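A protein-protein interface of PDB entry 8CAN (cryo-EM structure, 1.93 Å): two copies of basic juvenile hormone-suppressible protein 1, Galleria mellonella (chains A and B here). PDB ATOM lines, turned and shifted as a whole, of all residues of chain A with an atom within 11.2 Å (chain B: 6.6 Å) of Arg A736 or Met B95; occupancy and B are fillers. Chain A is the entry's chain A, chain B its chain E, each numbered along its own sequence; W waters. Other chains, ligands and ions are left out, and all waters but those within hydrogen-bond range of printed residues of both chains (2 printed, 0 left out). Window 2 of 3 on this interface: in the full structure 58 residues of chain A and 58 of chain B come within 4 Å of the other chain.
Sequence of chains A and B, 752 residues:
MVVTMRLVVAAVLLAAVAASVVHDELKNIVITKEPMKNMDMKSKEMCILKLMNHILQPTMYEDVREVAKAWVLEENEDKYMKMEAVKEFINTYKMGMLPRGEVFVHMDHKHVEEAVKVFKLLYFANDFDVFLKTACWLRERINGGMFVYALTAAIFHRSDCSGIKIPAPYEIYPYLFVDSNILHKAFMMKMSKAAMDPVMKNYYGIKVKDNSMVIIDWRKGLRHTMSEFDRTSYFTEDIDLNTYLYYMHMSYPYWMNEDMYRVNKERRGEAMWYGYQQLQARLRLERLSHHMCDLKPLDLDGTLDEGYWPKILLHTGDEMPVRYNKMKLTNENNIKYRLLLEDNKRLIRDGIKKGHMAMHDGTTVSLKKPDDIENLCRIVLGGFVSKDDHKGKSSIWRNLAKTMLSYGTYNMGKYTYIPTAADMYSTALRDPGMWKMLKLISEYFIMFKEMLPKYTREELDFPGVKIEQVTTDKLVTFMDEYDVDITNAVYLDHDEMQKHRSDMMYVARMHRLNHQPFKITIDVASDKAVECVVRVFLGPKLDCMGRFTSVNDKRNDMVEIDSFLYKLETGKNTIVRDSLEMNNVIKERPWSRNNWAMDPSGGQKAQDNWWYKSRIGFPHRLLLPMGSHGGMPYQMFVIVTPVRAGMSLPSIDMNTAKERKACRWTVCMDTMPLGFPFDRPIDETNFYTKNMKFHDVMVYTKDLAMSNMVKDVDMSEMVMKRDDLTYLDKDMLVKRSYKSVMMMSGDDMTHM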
ATOM      1  N   VAL A 713      37.434 -28.150  12.827  1.00  0.00           N
ATOM      2  CA  VAL A 713      36.011 -27.848  12.924  1.00  0.00           C
ATOM      3  C   VAL A 713      35.395 -27.951  11.535  1.00  0.00           C
ATOM      4  O   VAL A 713      36.030 -27.647  10.523  1.00  0.00           O
ATOM      5  CB  VAL A 713      35.748 -26.448  13.525  1.00  0.00           C
ATOM      6  CG1 VAL A 713      34.266 -26.108  13.468  1.00  0.00           C
ATOM      7  CG2 VAL A 713      36.247 -26.380  14.958  1.00  0.00           C
ATOM      8  N   ASP A 714      34.140 -28.386  11.500  1.00  0.00           N
ATOM      9  CA  ASP A 714      33.383 -28.507  10.263  1.00  0.00           C
ATOM     10  C   ASP A 714      32.593 -27.229  10.009  1.00  0.00           C
ATOM     11  O   ASP A 714      32.062 -26.610  10.934  1.00  0.00           O
ATOM     12  CB  ASP A 714      32.433 -29.705  10.320  1.00  0.00           C
ATOM     13  CG  ASP A 714      31.629 -29.871   9.046  1.00  0.00           C
ATOM     14  OD1 ASP A 714      32.230 -30.214   8.005  1.00  0.00           O
ATOM     15  OD2 ASP A 714      30.399 -29.658   9.084  1.00  0.00           O
ATOM     16  N   MET A 715      32.519 -26.841   8.732  1.00  0.00           N
ATOM     17  CA  MET A 715      31.878 -25.593   8.335  1.00  0.00           C
ATOM     18  C   MET A 715      30.732 -25.826   7.356  1.00  0.00           C
ATOM     19  O   MET A 715      30.412 -24.933   6.566  1.00  0.00           O
ATOM     20  CB  MET A 715      32.904 -24.636   7.722  1.00  0.00           C
ATOM     21  CG  MET A 715      33.528 -25.144   6.434  1.00  0.00           C
ATOM     22  SD  MET A 715      34.875 -24.092   5.864  1.00  0.00           S
ATOM     23  CE  MET A 715      35.272 -24.865   4.299  1.00  0.00           C
ATOM     24  N   SER A 716      30.105 -27.003   7.394  1.00  0.00           N
ATOM     25  CA  SER A 716      29.000 -27.284   6.486  1.00  0.00           C
ATOM     26  C   SER A 716      27.777 -26.424   6.780  1.00  0.00           C
ATOM     27  O   SER A 716      26.895 -26.312   5.923  1.00  0.00           O
ATOM     28  CB  SER A 716      28.622 -28.764   6.564  1.00  0.00           C
ATOM     29  OG  SER A 716      29.709 -29.591   6.183  1.00  0.00           O
ATOM     30  N   GLU A 717      27.703 -25.817   7.966  1.00  0.00           N
ATOM     31  CA  GLU A 717      26.553 -25.018   8.363  1.00  0.00           C
ATOM     32  C   GLU A 717      26.867 -23.534   8.503  1.00  0.00           C
ATOM     33  O   GLU A 717      25.973 -22.763   8.870  1.00  0.00           O
ATOM     34  CB  GLU A 717      25.977 -25.538   9.689  1.00  0.00           C
ATOM     35  CG  GLU A 717      25.500 -26.986   9.650  1.00  0.00           C
ATOM     36  CD  GLU A 717      26.642 -27.984   9.661  1.00  0.00           C
ATOM     37  OE1 GLU A 717      27.813 -27.552   9.614  1.00  0.00           O
ATOM     38  OE2 GLU A 717      26.369 -29.202   9.718  1.00  0.00           O
ATOM     39  N   MET A 718      28.097 -23.111   8.225  1.00  0.00           N
ATOM     40  CA  MET A 718      28.457 -21.708   8.349  1.00  0.00           C
ATOM     41  C   MET A 718      27.873 -20.900   7.191  1.00  0.00           C
ATOM     42  O   MET A 718      27.551 -21.430   6.125  1.00  0.00           O
ATOM     43  CB  MET A 718      29.977 -21.545   8.392  1.00  0.00           C
ATOM     44  CG  MET A 718      30.626 -22.180   9.612  1.00  0.00           C
ATOM     45  SD  MET A 718      32.412 -21.940   9.683  1.00  0.00           S
ATOM     46  CE  MET A 718      32.516 -20.170   9.939  1.00  0.00           C
ATOM     47  N   VAL A 719      27.743 -19.593   7.417  1.00  0.00           N
ATOM     48  CA  VAL A 719      27.168 -18.677   6.442  1.00  0.00           C
ATOM     49  C   VAL A 719      28.095 -17.481   6.276  1.00  0.00           C
ATOM     50  O   VAL A 719      28.865 -17.134   7.178  1.00  0.00           O
ATOM     51  CB  VAL A 719      25.752 -18.208   6.854  1.00  0.00           C
ATOM     52  CG1 VAL A 719      24.784 -19.381   6.861  1.00  0.00           C
ATOM     53  CG2 VAL A 719      25.784 -17.528   8.216  1.00  0.00           C
ATOM     54  N   MET A 720      28.015 -16.850   5.107  1.00  0.00           N
ATOM     55  CA  MET A 720      28.827 -15.676   4.826  1.00  0.00           C
ATOM     56  C   MET A 720      28.341 -14.474   5.629  1.00  0.00           C
ATOM     57  O   MET A 720      27.158 -14.354   5.960  1.00  0.00           O
ATOM     58  CB  MET A 720      28.789 -15.346   3.335  1.00  0.00           C
ATOM     59  CG  MET A 720      29.590 -16.295   2.464  1.00  0.00           C
ATOM     60  SD  MET A 720      31.366 -16.139   2.729  1.00  0.00           S
ATOM     61  CE  MET A 720      31.991 -17.336   1.555  1.00  0.00           C
ATOM     62  N   LYS A 721      29.276 -13.576   5.942  1.00  0.00           N
ATOM     63  CA  LYS A 721      28.910 -12.336   6.619  1.00  0.00           C
ATOM     64  C   LYS A 721      27.971 -11.502   5.755  1.00  0.00           C
ATOM     65  O   LYS A 721      26.997 -10.930   6.257  1.00  0.00           O
ATOM     66  CB  LYS A 721      30.169 -11.544   6.973  1.00  0.00           C
ATOM     67  CG  LYS A 721      29.909 -10.309   7.819  1.00  0.00           C
ATOM     68  CD  LYS A 721      31.208  -9.678   8.303  1.00  0.00           C
ATOM     69  CE  LYS A 721      32.035  -9.129   7.151  1.00  0.00           C
ATOM     70  NZ  LYS A 721      33.268  -8.444   7.627  1.00  0.00           N
ATOM     71  N   MET A 732      35.385 -15.004   5.125  1.00  0.00           N
ATOM     72  CA  MET A 732      34.276 -14.210   5.636  1.00  0.00           C
ATOM     73  C   MET A 732      33.141 -15.071   6.177  1.00  0.00           C
ATOM     74  O   MET A 732      32.100 -14.531   6.565  1.00  0.00           O
ATOM     75  CB  MET A 732      33.746 -13.285   4.538  1.00  0.00           C
ATOM     76  CG  MET A 732      34.718 -12.193   4.114  1.00  0.00           C
ATOM     77  SD  MET A 732      34.957 -10.920   5.374  1.00  0.00           S
ATOM     78  CE  MET A 732      36.486 -11.459   6.137  1.00  0.00           C
ATOM     79  N   LEU A 733      33.316 -16.390   6.217  1.00  0.00           N
ATOM     80  CA  LEU A 733      32.292 -17.277   6.747  1.00  0.00           C
ATOM     81  C   LEU A 733      32.235 -17.162   8.265  1.00  0.00           C
ATOM     82  O   LEU A 733      33.264 -17.246   8.943  1.00  0.00           O
ATOM     83  CB  LEU A 733      32.574 -18.723   6.340  1.00  0.00           C
ATOM     84  CG  LEU A 733      32.346 -19.081   4.871  1.00  0.00           C
ATOM     85  CD1 LEU A 733      32.911 -20.458   4.573  1.00  0.00           C
ATOM     86  CD2 LEU A 733      30.866 -19.026   4.530  1.00  0.00           C
ATOM     87  N   VAL A 734      31.029 -16.972   8.794  1.00  0.00           N
ATOM     88  CA  VAL A 734      30.789 -16.883  10.228  1.00  0.00           C
ATOM     89  C   VAL A 734      29.683 -17.863  10.589  1.00  0.00           C
ATOM     90  O   VAL A 734      28.648 -17.919   9.916  1.00  0.00           O
ATOM     91  CB  VAL A 734      30.412 -15.450  10.658  1.00  0.00           C
ATOM     92  CG1 VAL A 734      31.525 -14.476  10.306  1.00  0.00           C
ATOM     93  CG2 VAL A 734      29.101 -15.027  10.009  1.00  0.00           C
ATOM     94  N   LYS A 735      29.904 -18.636  11.648  1.00  0.00           N
ATOM     95  CA  LYS A 735      28.911 -19.612  12.072  1.00  0.00           C
ATOM     96  C   LYS A 735      27.627 -18.907  12.486  1.00  0.00           C
ATOM     97  O   LYS A 735      27.654 -17.838  13.103  1.00  0.00           O
ATOM     98  CB  LYS A 735      29.447 -20.454  13.229  1.00  0.00           C
ATOM     99  CG  LYS A 735      28.507 -21.567  13.684  1.00  0.00           C
ATOM    100  CD  LYS A 735      28.379 -22.665  12.635  1.00  0.00           C
ATOM    101  CE  LYS A 735      27.205 -23.583  12.929  1.00  0.00           C
ATOM    102  NZ  LYS A 735      25.894 -22.896  12.749  1.00  0.00           N
ATOM    103  N   ARG A 736      26.495 -19.512  12.141  1.00  0.00           N
ATOM    104  CA  ARG A 736      25.198 -18.929  12.452  1.00  0.00           C
ATOM    105  C   ARG A 736      25.049 -18.722  13.953  1.00  0.00           C
ATOM    106  O   ARG A 736      25.063 -19.683  14.728  1.00  0.00           O
ATOM    107  CB  ARG A 736      24.087 -19.837  11.925  1.00  0.00           C
ATOM    108  CG  ARG A 736      24.203 -20.153  10.445  1.00  0.00           C
ATOM    109  CD  ARG A 736      23.076 -21.065   9.987  1.00  0.00           C
ATOM    110  NE  ARG A 736      21.783 -20.389   9.971  1.00  0.00           N
ATOM    111  CZ  ARG A 736      20.617 -20.994   9.790  1.00  0.00           C
ATOM    112  NH1 ARG A 736      20.531 -22.305   9.629  1.00  0.00           N
ATOM    113  NH2 ARG A 736      19.506 -20.268   9.773  1.00  0.00           N
ATOM    114  N   SER A 737      24.901 -17.464  14.358  1.00  0.00           N
ATOM    115  CA  SER A 737      24.801 -17.085  15.759  1.00  0.00           C
ATOM    116  C   SER A 737      23.356 -16.759  16.116  1.00  0.00           C
ATOM    117  O   SER A 737      22.480 -16.659  15.253  1.00  0.00           O
ATOM    118  CB  SER A 737      25.705 -15.884  16.063  1.00  0.00           C
ATOM    119  OG  SER A 737      25.315 -14.747  15.313  1.00  0.00           O
ATOM    120  N   TYR A 738      23.117 -16.594  17.416  1.00  0.00           N
ATOM    121  CA  TYR A 738      21.802 -16.253  17.943  1.00  0.00           C
ATOM    122  C   TYR A 738      21.937 -15.022  18.826  1.00  0.00           C
ATOM    123  O   TYR A 738      22.643 -15.058  19.839  1.00  0.00           O
ATOM    124  CB  TYR A 738      21.205 -17.422  18.735  1.00  0.00           C
ATOM    125  CG  TYR A 738      21.082 -18.699  17.934  1.00  0.00           C
ATOM    126  CD1 TYR A 738      22.152 -19.577  17.821  1.00  0.00           C
ATOM    127  CD2 TYR A 738      19.895 -19.026  17.291  1.00  0.00           C
ATOM    128  CE1 TYR A 738      22.044 -20.745  17.090  1.00  0.00           C
ATOM    129  CE2 TYR A 738      19.778 -20.191  16.557  1.00  0.00           C
ATOM    130  CZ  TYR A 738      20.855 -21.046  16.461  1.00  0.00           C
ATOM    131  OH  TYR A 738      20.744 -22.208  15.732  1.00  0.00           O
ATOM    132  N   LYS A 739      21.260 -13.943  18.446  1.00  0.00           N
ATOM    133  CA  LYS A 739      21.319 -12.694  19.197  1.00  0.00           C
ATOM    134  C   LYS A 739      20.351 -12.724  20.375  1.00  0.00           C
ATOM    135  O   LYS A 739      20.418 -13.611  21.224  1.00  0.00           O
ATOM    136  CB  LYS A 739      21.002 -11.506  18.287  1.00  0.00           C
ATOM    137  CG  LYS A 739      21.986 -11.317  17.143  1.00  0.00           C
ATOM    138  CD  LYS A 739      21.604 -10.131  16.271  1.00  0.00           C
ATOM    139  CE  LYS A 739      22.595  -9.930  15.136  1.00  0.00           C
ATOM    140  NZ  LYS A 739      22.209  -8.790  14.261  1.00  0.00           N
ATOM    141  N   ILE B  90      10.754 -11.984  18.432  1.00  0.00           N
ATOM    142  CA  ILE B  90      11.947 -12.414  19.158  1.00  0.00           C
ATOM    143  C   ILE B  90      12.650 -13.533  18.403  1.00  0.00           C
ATOM    144  O   ILE B  90      13.878 -13.524  18.251  1.00  0.00           O
ATOM    145  CB  ILE B  90      11.577 -12.838  20.592  1.00  0.00           C
ATOM    146  CG1 ILE B  90      11.153 -11.613  21.408  1.00  0.00           C
ATOM    147  CG2 ILE B  90      12.752 -13.552  21.253  1.00  0.00           C
ATOM    148  CD1 ILE B  90      10.603 -11.943  22.780  1.00  0.00           C
ATOM    149  N   ASN B  91      11.886 -14.515  17.918  1.00  0.00           N
ATOM    150  CA  ASN B  91      12.494 -15.613  17.170  1.00  0.00           C
ATOM    151  C   ASN B  91      13.177 -15.101  15.907  1.00  0.00           C
ATOM    152  O   ASN B  91      14.320 -15.473  15.606  1.00  0.00           O
ATOM    153  CB  ASN B  91      11.432 -16.658  16.825  1.00  0.00           C
ATOM    154  CG  ASN B  91      10.802 -17.277  18.056  1.00  0.00           C
ATOM    155  OD1 ASN B  91      11.451 -17.428  19.091  1.00  0.00           O
ATOM    156  ND2 ASN B  91       9.528 -17.638  17.950  1.00  0.00           N
ATOM    157  N   THR B  92      12.497 -14.226  15.160  1.00  0.00           N
ATOM    158  CA  THR B  92      13.076 -13.706  13.926  1.00  0.00           C
ATOM    159  C   THR B  92      14.342 -12.905  14.207  1.00  0.00           C
ATOM    160  O   THR B  92      15.339 -13.034  13.487  1.00  0.00           O
ATOM    161  CB  THR B  92      12.047 -12.846  13.190  1.00  0.00           C
ATOM    162  OG1 THR B  92      10.875 -13.625  12.919  1.00  0.00           O
ATOM    163  CG2 THR B  92      12.618 -12.328  11.878  1.00  0.00           C
ATOM    164  N   TYR B  93      14.323 -12.073  15.251  1.00  0.00           N
ATOM    165  CA  TYR B  93      15.500 -11.286  15.598  1.00  0.00           C
ATOM    166  C   TYR B  93      16.660 -12.184  16.000  1.00  0.00           C
ATOM    167  O   TYR B  93      17.807 -11.944  15.602  1.00  0.00           O
ATOM    168  CB  TYR B  93      15.159 -10.309  16.722  1.00  0.00           C
ATOM    169  CG  TYR B  93      16.330  -9.475  17.187  1.00  0.00           C
ATOM    170  CD1 TYR B  93      16.727  -8.346  16.483  1.00  0.00           C
ATOM    171  CD2 TYR B  93      17.036  -9.812  18.334  1.00  0.00           C
ATOM    172  CE1 TYR B  93      17.795  -7.581  16.905  1.00  0.00           C
ATOM    173  CE2 TYR B  93      18.106  -9.053  18.764  1.00  0.00           C
ATOM    174  CZ  TYR B  93      18.482  -7.938  18.046  1.00  0.00           C
ATOM    175  OH  TYR B  93      19.547  -7.178  18.470  1.00  0.00           O
ATOM    176  N   LYS B  94      16.386 -13.225  16.790  1.00  0.00           N
ATOM    177  CA  LYS B  94      17.439 -14.170  17.142  1.00  0.00           C
ATOM    178  C   LYS B  94      17.996 -14.864  15.907  1.00  0.00           C
ATOM    179  O   LYS B  94      19.189 -15.180  15.859  1.00  0.00           O
ATOM    180  CB  LYS B  94      16.913 -15.201  18.140  1.00  0.00           C
ATOM    181  CG  LYS B  94      16.707 -14.652  19.542  1.00  0.00           C
ATOM    182  CD  LYS B  94      16.280 -15.744  20.509  1.00  0.00           C
ATOM    183  CE  LYS B  94      16.198 -15.225  21.936  1.00  0.00           C
ATOM    184  NZ  LYS B  94      17.522 -14.770  22.440  1.00  0.00           N
ATOM    185  N   MET B  95      17.154 -15.106  14.900  1.00  0.00           N
ATOM    186  CA  MET B  95      17.623 -15.712  13.661  1.00  0.00           C
ATOM    187  C   MET B  95      18.327 -14.723  12.740  1.00  0.00           C
ATOM    188  O   MET B  95      18.908 -15.148  11.736  1.00  0.00           O
ATOM    189  CB  MET B  95      16.451 -16.356  12.916  1.00  0.00           C
ATOM    190  CG  MET B  95      15.909 -17.612  13.580  1.00  0.00           C
ATOM    191  SD  MET B  95      17.082 -18.983  13.581  1.00  0.00           S
ATOM    192  CE  MET B  95      17.244 -19.302  11.825  1.00  0.00           C
ATOM    193  N   GLY B  96      18.292 -13.429  13.050  1.00  0.00           N
ATOM    194  CA  GLY B  96      18.948 -12.433  12.224  1.00  0.00           C
ATOM    195  C   GLY B  96      17.995 -11.711  11.293  1.00  0.00           C
ATOM    196  O   GLY B  96      17.074 -12.321  10.743  1.00  0.00           O
ATOM    197  N   MET B  97      18.205 -10.411  11.112  1.00  0.00           N
ATOM    198  CA  MET B  97      17.359  -9.574  10.271  1.00  0.00           C
ATOM    199  C   MET B  97      18.233  -8.752   9.323  1.00  0.00           C
ATOM    200  O   MET B  97      19.447  -8.958   9.222  1.00  0.00           O
ATOM    201  CB  MET B  97      16.470  -8.681  11.141  1.00  0.00           C
ATOM    202  CG  MET B  97      15.506  -9.450  12.030  1.00  0.00           C
ATOM    203  SD  MET B  97      14.530  -8.383  13.109  1.00  0.00           S
ATOM    204  CE  MET B  97      13.609  -7.425  11.909  1.00  0.00           C
ATOM    205  N   TYR B 415      19.194  -9.520   1.084  1.00  0.00           N
ATOM    206  CA  TYR B 415      19.504  -8.300   1.819  1.00  0.00           C
ATOM    207  C   TYR B 415      20.349  -7.322   1.015  1.00  0.00           C
ATOM    208  O   TYR B 415      20.439  -6.151   1.401  1.00  0.00           O
ATOM    209  CB  TYR B 415      20.236  -8.642   3.121  1.00  0.00           C
ATOM    210  CG  TYR B 415      19.421  -9.423   4.132  1.00  0.00           C
ATOM    211  CD1 TYR B 415      18.037  -9.317   4.181  1.00  0.00           C
ATOM    212  CD2 TYR B 415      20.044 -10.261   5.047  1.00  0.00           C
ATOM    213  CE1 TYR B 415      17.298 -10.028   5.109  1.00  0.00           C
ATOM    214  CE2 TYR B 415      19.315 -10.975   5.976  1.00  0.00           C
ATOM    215  CZ  TYR B 415      17.943 -10.856   6.003  1.00  0.00           C
ATOM    216  OH  TYR B 415      17.215 -11.565   6.929  1.00  0.00           O
HETATM  217  O   HOH W   1      18.920  -9.479  14.029  1.00  0.00           O
HETATM  218  O   HOH W   2      20.807  -6.285  15.823  1.00  0.00           O
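Water W2 bridges OH of Tyr B93 and NZ of Lys A739. Water W1 lies within hydrogen-bond range of the backbone carbonyl oxygen (O) of Tyr B93 (3.1 Å), the backbone NH (N) of Met B97 (3.1 Å) and the side-chain amino group (NZ) of Lys A739 (3.4 Å).
Met B95 touches just one residue of chain A: Arg A736 (3.2 Å). Thr B92 touches none of the printed residues of chain A. Printed residues of chain B within 4 Å of Lys A739: Tyr B93 (3.8 Å) and Lys B94 (3.3 Å). Printed residues of chain A within 4 Å of Tyr B93: Lys A739. Lys A735 touches none of the printed residues of chain B. Val A734 touches none of the printed residues of chain B. The nearest residue of chain A that does not touch Met B95 is Tyr A738 (4.2 Å).
Of the 17 printed residues of chain A, 4 touch a printed residue of chain B. Among the printed residues, 5 pairs touch across the chains. Among the printed residues, no Asp or Glu carboxylate lies within 4 Å of a Lys or Arg side-chain nitrogen of the other chain.
Among the printed residues, merely in contact across the chains: Arg A736 with Met B95, Tyr A738 with Lys B94, Ser A737 with Lys B94 and Lys A739 with Tyr B93.
No position is printed for both chains. Of the 5 pairs that touch across the chains among the printed residues, none has its exchanged pair printed and touching as well.
O of Lys A739 is in hydrogen-bond range of NZ of Lys B94 (3.3 Å).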
